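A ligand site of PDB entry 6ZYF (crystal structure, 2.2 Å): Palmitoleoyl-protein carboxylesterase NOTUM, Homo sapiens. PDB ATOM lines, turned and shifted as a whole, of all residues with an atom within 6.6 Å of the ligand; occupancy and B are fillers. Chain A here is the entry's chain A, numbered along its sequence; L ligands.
The backbone NH (N) of Ala 156 sits at hydrogen-bond distance from an oxygen (O1) of the ligand, at 2.9 Å.
NE2 of His 312 lies within hydrogen-bond range of O2 of the ligand.
An oxygen (O1) of the ligand lies within hydrogen-bond range of the backbone NH (N) of Trp 51, at 3.1 Å.
O of Trp 51 is in hydrogen-bond range of OH of Tyr 105 (2.9 Å).
The side-chain hydroxyl of Ser 188 sits at hydrogen-bond distance from the backbone NH of Glu 313.
A ring nitrogen (ND1) of His 312 is in hydrogen-bond range of the side-chain carboxylate (OD2) of Asp 263 (3.0 Å).
O3 of the ligand lies close to OE2 of Glu 313 (2.8 Å).
Gly 49 touches the ligand (C to O3, 3.7 Å).
Gly 50 touches the ligand.
Tyr 52 touches the ligand (CE1 to C4, 3.6 Å).
Ala 155 touches the ligand (CB to O1, 3.4 Å).
Phe 191 touches the ligand (CD2 to C3, 3.5 Å).
CD1 of Ile 214 touches C2 of the ligand (3.8 Å).
Phe 242 touches the ligand (O to C1, 3.98 Å).
CE1 of Phe 243 touches C1 of the ligand (3.7 Å).
Hydrophobic or aromatic side chains that line the ligand: Trp 51, Tyr 52, Ala 155, Ala 156, Phe 191, Ile 214, Phe 243 and His 312.
Along chain A the residues within 4 Å of the ligand span positions 49 to 313.
The nearest printed residue that does not touch the ligand is Ala 265 (4.03 Å).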
ATOM      1  N   GLU A  48     -25.016  12.175  -4.954  1.00  0.00           N
ATOM      2  CA  GLU A  48     -23.945  12.931  -5.589  1.00  0.00           C
ATOM      3  C   GLU A  48     -24.497  13.885  -6.639  1.00  0.00           C
ATOM      4  O   GLU A  48     -25.577  13.667  -7.196  1.00  0.00           O
ATOM      5  CB  GLU A  48     -22.946  11.960  -6.224  1.00  0.00           C
ATOM      6  CG  GLU A  48     -21.663  12.584  -6.742  1.00  0.00           C
ATOM      7  CD  GLU A  48     -20.775  11.579  -7.452  1.00  0.00           C
ATOM      8  OE1 GLU A  48     -21.303  10.595  -8.000  1.00  0.00           O
ATOM      9  OE2 GLU A  48     -19.538  11.766  -7.444  1.00  0.00           O
ATOM     10  N   GLY A  49     -23.752  14.950  -6.901  1.00  0.00           N
ATOM     11  CA  GLY A  49     -24.120  15.937  -7.887  1.00  0.00           C
ATOM     12  C   GLY A  49     -23.281  15.838  -9.144  1.00  0.00           C
ATOM     13  O   GLY A  49     -22.589  14.829  -9.394  1.00  0.00           O
ATOM     14  N   GLY A  50     -23.327  16.889  -9.962  1.00  0.00           N
ATOM     15  CA  GLY A  50     -22.568  16.915 -11.197  1.00  0.00           C
ATOM     16  C   GLY A  50     -23.332  17.364 -12.425  1.00  0.00           C
ATOM     17  O   GLY A  50     -23.266  16.714 -13.473  1.00  0.00           O
ATOM     18  N   TRP A  51     -24.065  18.466 -12.298  1.00  0.00           N
ATOM     19  CA  TRP A  51     -24.746  19.136 -13.426  1.00  0.00           C
ATOM     20  C   TRP A  51     -25.736  18.155 -14.066  1.00  0.00           C
ATOM     21  O   TRP A  51     -26.396  17.389 -13.341  1.00  0.00           O
ATOM     22  CB  TRP A  51     -23.727  19.719 -14.377  1.00  0.00           C
ATOM     23  CG  TRP A  51     -23.017  20.928 -13.850  1.00  0.00           C
ATOM     24  CD1 TRP A  51     -21.787  20.966 -13.249  1.00  0.00           C
ATOM     25  CD2 TRP A  51     -23.501  22.275 -13.864  1.00  0.00           C
ATOM     26  NE1 TRP A  51     -21.475  22.256 -12.896  1.00  0.00           N
ATOM     27  CE2 TRP A  51     -22.511  23.079 -13.256  1.00  0.00           C
ATOM     28  CE3 TRP A  51     -24.671  22.882 -14.323  1.00  0.00           C
ATOM     29  CZ2 TRP A  51     -22.663  24.454 -13.109  1.00  0.00           C
ATOM     30  CZ3 TRP A  51     -24.813  24.247 -14.170  1.00  0.00           C
ATOM     31  CH2 TRP A  51     -23.814  25.016 -13.567  1.00  0.00           C
ATOM     32  N   TYR A  52     -25.833  18.151 -15.396  1.00  0.00           N
ATOM     33  CA  TYR A  52     -26.893  17.463 -16.130  1.00  0.00           C
ATOM     34  C   TYR A  52     -26.679  17.624 -17.624  1.00  0.00           C
ATOM     35  O   TYR A  52     -25.722  18.286 -18.046  1.00  0.00           O
ATOM     36  CB  TYR A  52     -28.266  18.008 -15.730  1.00  0.00           C
ATOM     37  CG  TYR A  52     -28.325  19.527 -15.634  1.00  0.00           C
ATOM     38  CD1 TYR A  52     -28.286  20.169 -14.404  1.00  0.00           C
ATOM     39  CD2 TYR A  52     -28.404  20.311 -16.779  1.00  0.00           C
ATOM     40  CE1 TYR A  52     -28.327  21.550 -14.323  1.00  0.00           C
ATOM     41  CE2 TYR A  52     -28.444  21.688 -16.707  1.00  0.00           C
ATOM     42  CZ  TYR A  52     -28.408  22.302 -15.465  1.00  0.00           C
ATOM     43  OH  TYR A  52     -28.440  23.673 -15.378  1.00  0.00           O
ATOM     44  N   TYR A 105     -23.804   9.585  -8.973  1.00  0.00           N
ATOM     45  CA  TYR A 105     -24.683  10.279  -9.906  1.00  0.00           C
ATOM     46  C   TYR A 105     -24.304   9.877 -11.331  1.00  0.00           C
ATOM     47  O   TYR A 105     -23.268  10.323 -11.857  1.00  0.00           O
ATOM     48  CB  TYR A 105     -24.555  11.793  -9.708  1.00  0.00           C
ATOM     49  CG  TYR A 105     -25.495  12.649 -10.532  1.00  0.00           C
ATOM     50  CD1 TYR A 105     -26.841  12.323 -10.658  1.00  0.00           C
ATOM     51  CD2 TYR A 105     -25.031  13.807 -11.146  1.00  0.00           C
ATOM     52  CE1 TYR A 105     -27.693  13.118 -11.401  1.00  0.00           C
ATOM     53  CE2 TYR A 105     -25.874  14.602 -11.888  1.00  0.00           C
ATOM     54  CZ  TYR A 105     -27.209  14.262 -12.018  1.00  0.00           C
ATOM     55  OH  TYR A 105     -28.042  15.057 -12.758  1.00  0.00           O
ATOM     56  N   VAL A 110     -30.816  15.217 -12.608  1.00  0.00           N
ATOM     57  CA  VAL A 110     -31.090  15.817 -11.312  1.00  0.00           C
ATOM     58  C   VAL A 110     -31.951  14.862 -10.485  1.00  0.00           C
ATOM     59  O   VAL A 110     -32.832  15.286  -9.727  1.00  0.00           O
ATOM     60  CB  VAL A 110     -31.755  17.198 -11.463  1.00  0.00           C
ATOM     61  CG1 VAL A 110     -31.596  18.023 -10.189  1.00  0.00           C
ATOM     62  CG2 VAL A 110     -31.153  17.959 -12.644  1.00  0.00           C
ATOM     63  N   SER A 154     -25.593  16.958  -2.409  1.00  0.00           N
ATOM     64  CA  SER A 154     -24.887  18.192  -2.718  1.00  0.00           C
ATOM     65  C   SER A 154     -25.115  18.567  -4.187  1.00  0.00           C
ATOM     66  O   SER A 154     -25.089  17.698  -5.066  1.00  0.00           O
ATOM     67  CB  SER A 154     -23.383  18.064  -2.449  1.00  0.00           C
ATOM     68  OG  SER A 154     -23.113  18.068  -1.054  1.00  0.00           O
ATOM     69  N   ALA A 155     -25.326  19.858  -4.428  1.00  0.00           N
ATOM     70  CA  ALA A 155     -25.454  20.430  -5.772  1.00  0.00           C
ATOM     71  C   ALA A 155     -26.651  19.764  -6.456  1.00  0.00           C
ATOM     72  O   ALA A 155     -27.773  19.862  -5.927  1.00  0.00           O
ATOM     73  CB  ALA A 155     -24.114  20.307  -6.494  1.00  0.00           C
ATOM     74  N   ALA A 156     -26.470  19.104  -7.606  1.00  0.00           N
ATOM     75  CA  ALA A 156     -27.583  18.407  -8.244  1.00  0.00           C
ATOM     76  C   ALA A 156     -28.209  17.378  -7.311  1.00  0.00           C
ATOM     77  O   ALA A 156     -29.408  17.126  -7.385  1.00  0.00           O
ATOM     78  CB  ALA A 156     -27.119  17.736  -9.539  1.00  0.00           C
ATOM     79  N   GLY A 157     -27.399  16.773  -6.437  1.00  0.00           N
ATOM     80  CA  GLY A 157     -27.950  15.877  -5.432  1.00  0.00           C
ATOM     81  C   GLY A 157     -28.773  16.597  -4.379  1.00  0.00           C
ATOM     82  O   GLY A 157     -29.707  16.026  -3.818  1.00  0.00           O
ATOM     83  N   THR A 159     -30.685  19.313  -5.011  1.00  0.00           N
ATOM     84  CA  THR A 159     -31.982  19.451  -5.675  1.00  0.00           C
ATOM     85  C   THR A 159     -32.708  18.118  -5.754  1.00  0.00           C
ATOM     86  O   THR A 159     -33.935  18.063  -5.655  1.00  0.00           O
ATOM     87  CB  THR A 159     -31.800  20.050  -7.069  1.00  0.00           C
ATOM     88  OG1 THR A 159     -31.018  21.247  -6.990  1.00  0.00           O
ATOM     89  CG2 THR A 159     -33.146  20.380  -7.703  1.00  0.00           C
ATOM     90  N   SER A 188     -26.493  23.094  -1.389  1.00  0.00           N
ATOM     91  CA  SER A 188     -26.184  23.755  -2.662  1.00  0.00           C
ATOM     92  C   SER A 188     -27.153  23.360  -3.766  1.00  0.00           C
ATOM     93  O   SER A 188     -26.788  23.315  -4.942  1.00  0.00           O
ATOM     94  CB  SER A 188     -24.739  23.466  -3.089  1.00  0.00           C
ATOM     95  OG  SER A 188     -23.818  24.180  -2.296  1.00  0.00           O
ATOM     96  N   GLY A 189     -28.404  23.070  -3.402  1.00  0.00           N
ATOM     97  CA  GLY A 189     -29.419  22.709  -4.383  1.00  0.00           C
ATOM     98  C   GLY A 189     -30.594  23.657  -4.376  1.00  0.00           C
ATOM     99  O   GLY A 189     -31.672  23.334  -4.899  1.00  0.00           O
ATOM    100  N   PHE A 191     -31.771  26.981  -5.731  1.00  0.00           N
ATOM    101  CA  PHE A 191     -31.452  27.913  -6.803  1.00  0.00           C
ATOM    102  C   PHE A 191     -32.615  28.851  -7.098  1.00  0.00           C
ATOM    103  O   PHE A 191     -33.760  28.615  -6.689  1.00  0.00           O
ATOM    104  CB  PHE A 191     -31.063  27.157  -8.082  1.00  0.00           C
ATOM    105  CG  PHE A 191     -29.824  26.329  -7.946  1.00  0.00           C
ATOM    106  CD1 PHE A 191     -28.576  26.924  -7.928  1.00  0.00           C
ATOM    107  CD2 PHE A 191     -29.902  24.949  -7.823  1.00  0.00           C
ATOM    108  CE1 PHE A 191     -27.425  26.157  -7.797  1.00  0.00           C
ATOM    109  CE2 PHE A 191     -28.761  24.182  -7.694  1.00  0.00           C
ATOM    110  CZ  PHE A 191     -27.523  24.786  -7.681  1.00  0.00           C
ATOM    111  N   LEU A 192     -32.302  29.928  -7.806  1.00  0.00           N
ATOM    112  CA  LEU A 192     -33.282  30.920  -8.244  1.00  0.00           C
ATOM    113  C   LEU A 192     -33.446  30.866  -9.758  1.00  0.00           C
ATOM    114  O   LEU A 192     -32.467  30.756 -10.498  1.00  0.00           O
ATOM    115  CB  LEU A 192     -32.853  32.334  -7.832  1.00  0.00           C
ATOM    116  CG  LEU A 192     -32.537  32.575  -6.358  1.00  0.00           C
ATOM    117  CD1 LEU A 192     -32.010  33.985  -6.140  1.00  0.00           C
ATOM    118  CD2 LEU A 192     -33.758  32.315  -5.486  1.00  0.00           C
ATOM    119  N   PRO A 210     -31.404  29.096 -16.000  1.00  0.00           N
ATOM    120  CA  PRO A 210     -31.973  27.996 -15.194  1.00  0.00           C
ATOM    121  C   PRO A 210     -33.371  27.580 -15.618  1.00  0.00           C
ATOM    122  O   PRO A 210     -33.661  26.380 -15.678  1.00  0.00           O
ATOM    123  CB  PRO A 210     -31.964  28.561 -13.770  1.00  0.00           C
ATOM    124  CG  PRO A 210     -30.967  29.670 -13.800  1.00  0.00           C
ATOM    125  CD  PRO A 210     -31.010  30.241 -15.177  1.00  0.00           C
ATOM    126  N   ILE A 214     -34.294  23.676 -17.287  1.00  0.00           N
ATOM    127  CA  ILE A 214     -35.195  22.703 -16.688  1.00  0.00           C
ATOM    128  C   ILE A 214     -36.411  22.440 -17.584  1.00  0.00           C
ATOM    129  O   ILE A 214     -36.902  21.306 -17.633  1.00  0.00           O
ATOM    130  CB  ILE A 214     -35.620  23.166 -15.285  1.00  0.00           C
ATOM    131  CG1 ILE A 214     -34.392  23.385 -14.412  1.00  0.00           C
ATOM    132  CG2 ILE A 214     -36.538  22.137 -14.643  1.00  0.00           C
ATOM    133  CD1 ILE A 214     -33.522  22.156 -14.247  1.00  0.00           C
ATOM    134  N   PHE A 242     -38.594  22.241  -9.595  1.00  0.00           N
ATOM    135  CA  PHE A 242     -37.164  22.028  -9.463  1.00  0.00           C
ATOM    136  C   PHE A 242     -36.481  23.108  -8.630  1.00  0.00           C
ATOM    137  O   PHE A 242     -35.278  22.991  -8.372  1.00  0.00           O
ATOM    138  CB  PHE A 242     -36.500  21.961 -10.834  1.00  0.00           C
ATOM    139  CG  PHE A 242     -36.560  20.606 -11.489  1.00  0.00           C
ATOM    140  CD1 PHE A 242     -37.770  20.043 -11.835  1.00  0.00           C
ATOM    141  CD2 PHE A 242     -35.390  19.915 -11.763  1.00  0.00           C
ATOM    142  CE1 PHE A 242     -37.814  18.796 -12.437  1.00  0.00           C
ATOM    143  CE2 PHE A 242     -35.434  18.669 -12.365  1.00  0.00           C
ATOM    144  CZ  PHE A 242     -36.646  18.109 -12.702  1.00  0.00           C
ATOM    145  N   PHE A 243     -37.204  24.145  -8.220  1.00  0.00           N
ATOM    146  CA  PHE A 243     -36.626  25.304  -7.556  1.00  0.00           C
ATOM    147  C   PHE A 243     -37.071  25.321  -6.103  1.00  0.00           C
ATOM    148  O   PHE A 243     -38.274  25.291  -5.813  1.00  0.00           O
ATOM    149  CB  PHE A 243     -37.011  26.586  -8.288  1.00  0.00           C
ATOM    150  CG  PHE A 243     -36.355  26.728  -9.631  1.00  0.00           C
ATOM    151  CD1 PHE A 243     -35.118  27.331  -9.749  1.00  0.00           C
ATOM    152  CD2 PHE A 243     -36.968  26.219 -10.771  1.00  0.00           C
ATOM    153  CE1 PHE A 243     -34.507  27.446 -10.987  1.00  0.00           C
ATOM    154  CE2 PHE A 243     -36.357  26.334 -12.009  1.00  0.00           C
ATOM    155  CZ  PHE A 243     -35.122  26.954 -12.113  1.00  0.00           C
ATOM    156  N   ASP A 263     -23.832  31.283  -4.446  1.00  0.00           N
ATOM    157  CA  ASP A 263     -23.428  29.976  -4.943  1.00  0.00           C
ATOM    158  C   ASP A 263     -22.767  30.115  -6.316  1.00  0.00           C
ATOM    159  O   ASP A 263     -23.290  30.813  -7.194  1.00  0.00           O
ATOM    160  CB  ASP A 263     -24.628  29.038  -5.013  1.00  0.00           C
ATOM    161  CG  ASP A 263     -24.233  27.605  -5.324  1.00  0.00           C
ATOM    162  OD1 ASP A 263     -23.918  27.309  -6.485  1.00  0.00           O
ATOM    163  OD2 ASP A 263     -24.248  26.776  -4.380  1.00  0.00           O
ATOM    164  N   ALA A 265     -22.284  27.836  -8.663  1.00  0.00           N
ATOM    165  CA  ALA A 265     -23.040  27.211  -9.749  1.00  0.00           C
ATOM    166  C   ALA A 265     -24.208  28.098 -10.165  1.00  0.00           C
ATOM    167  O   ALA A 265     -24.566  28.146 -11.353  1.00  0.00           O
ATOM    168  CB  ALA A 265     -23.524  25.831  -9.326  1.00  0.00           C
ATOM    169  N   GLN A 266     -24.817  28.791  -9.205  1.00  0.00           N
ATOM    170  CA  GLN A 266     -25.875  29.742  -9.526  1.00  0.00           C
ATOM    171  C   GLN A 266     -25.345  30.869 -10.404  1.00  0.00           C
ATOM    172  O   GLN A 266     -26.010  31.317 -11.333  1.00  0.00           O
ATOM    173  CB  GLN A 266     -26.482  30.301  -8.243  1.00  0.00           C
ATOM    174  CG  GLN A 266     -27.400  31.501  -8.435  1.00  0.00           C
ATOM    175  CD  GLN A 266     -28.776  31.107  -8.931  1.00  0.00           C
ATOM    176  OE1 GLN A 266     -29.427  30.229  -8.364  1.00  0.00           O
ATOM    177  NE2 GLN A 266     -29.235  31.764  -9.992  1.00  0.00           N
ATOM    178  N   VAL A 269     -24.770  29.523 -14.225  1.00  0.00           N
ATOM    179  CA  VAL A 269     -25.943  29.521 -15.088  1.00  0.00           C
ATOM    180  C   VAL A 269     -26.452  30.935 -15.333  1.00  0.00           C
ATOM    181  O   VAL A 269     -27.199  31.167 -16.299  1.00  0.00           O
ATOM    182  CB  VAL A 269     -27.061  28.652 -14.496  1.00  0.00           C
ATOM    183  CG1 VAL A 269     -26.652  27.190 -14.485  1.00  0.00           C
ATOM    184  CG2 VAL A 269     -27.435  29.118 -13.099  1.00  0.00           C
ATOM    185  N   HIS A 312     -19.313  26.488  -3.254  1.00  0.00           N
ATOM    186  CA  HIS A 312     -20.258  25.508  -3.780  1.00  0.00           C
ATOM    187  C   HIS A 312     -19.981  24.177  -3.083  1.00  0.00           C
ATOM    188  O   HIS A 312     -18.849  23.702  -3.116  1.00  0.00           O
ATOM    189  CB  HIS A 312     -20.100  25.367  -5.303  1.00  0.00           C
ATOM    190  CG  HIS A 312     -21.136  24.517  -5.951  1.00  0.00           C
ATOM    191  ND1 HIS A 312     -22.486  24.681  -5.722  1.00  0.00           N
ATOM    192  CD2 HIS A 312     -21.033  23.498  -6.833  1.00  0.00           C
ATOM    193  CE1 HIS A 312     -23.161  23.795  -6.430  1.00  0.00           C
ATOM    194  NE2 HIS A 312     -22.299  23.067  -7.112  1.00  0.00           N
ATOM    195  N   GLU A 313     -21.016  23.613  -2.450  1.00  0.00           N
ATOM    196  CA  GLU A 313     -20.950  22.326  -1.746  1.00  0.00           C
ATOM    197  C   GLU A 313     -20.136  22.428  -0.467  1.00  0.00           C
ATOM    198  O   GLU A 313     -19.255  23.286  -0.369  1.00  0.00           O
ATOM    199  CB  GLU A 313     -20.381  21.231  -2.655  1.00  0.00           C
ATOM    200  CG  GLU A 313     -21.267  20.861  -3.836  1.00  0.00           C
ATOM    201  CD  GLU A 313     -20.630  19.804  -4.721  1.00  0.00           C
ATOM    202  OE1 GLU A 313     -19.435  19.963  -5.068  1.00  0.00           O
ATOM    203  OE2 GLU A 313     -21.318  18.825  -5.061  1.00  0.00           O
HETATM  204  C1  LIG L   1     -32.395  24.471 -10.689  1.00  0.00           C
HETATM  205  C2  LIG L   1     -31.432  23.453 -11.286  1.00  0.00           C
HETATM  206  C3  LIG L   1     -29.979  23.890 -11.184  1.00  0.00           C
HETATM  207  C4  LIG L   1     -29.026  22.705 -11.026  1.00  0.00           C
HETATM  208  C5  LIG L   1     -27.560  23.121 -10.946  1.00  0.00           C
HETATM  209  C6  LIG L   1     -26.674  21.957 -10.521  1.00  0.00           C
HETATM  210  C7  LIG L   1     -25.196  22.326 -10.397  1.00  0.00           C
HETATM  211  C8  LIG L   1     -24.370  21.142  -9.905  1.00  0.00           C
HETATM  212  C9  LIG L   1     -22.293  20.098  -9.667  1.00  0.00           C
HETATM  213  C10 LIG L   1     -20.928  20.253  -8.991  1.00  0.00           C
HETATM  214  C11 LIG L   1     -20.369  18.870  -8.665  1.00  0.00           C
HETATM  215  N1  LIG L   1     -20.024  20.943  -9.893  1.00  0.00           N
HETATM  216  O1  LIG L   1     -24.872  20.076  -9.797  1.00  0.00           O
HETATM  217  O2  LIG L   1     -23.006  21.296  -9.590  1.00  0.00           O
HETATM  218  O3  LIG L   1     -20.797  18.250  -7.754  1.00  0.00           O
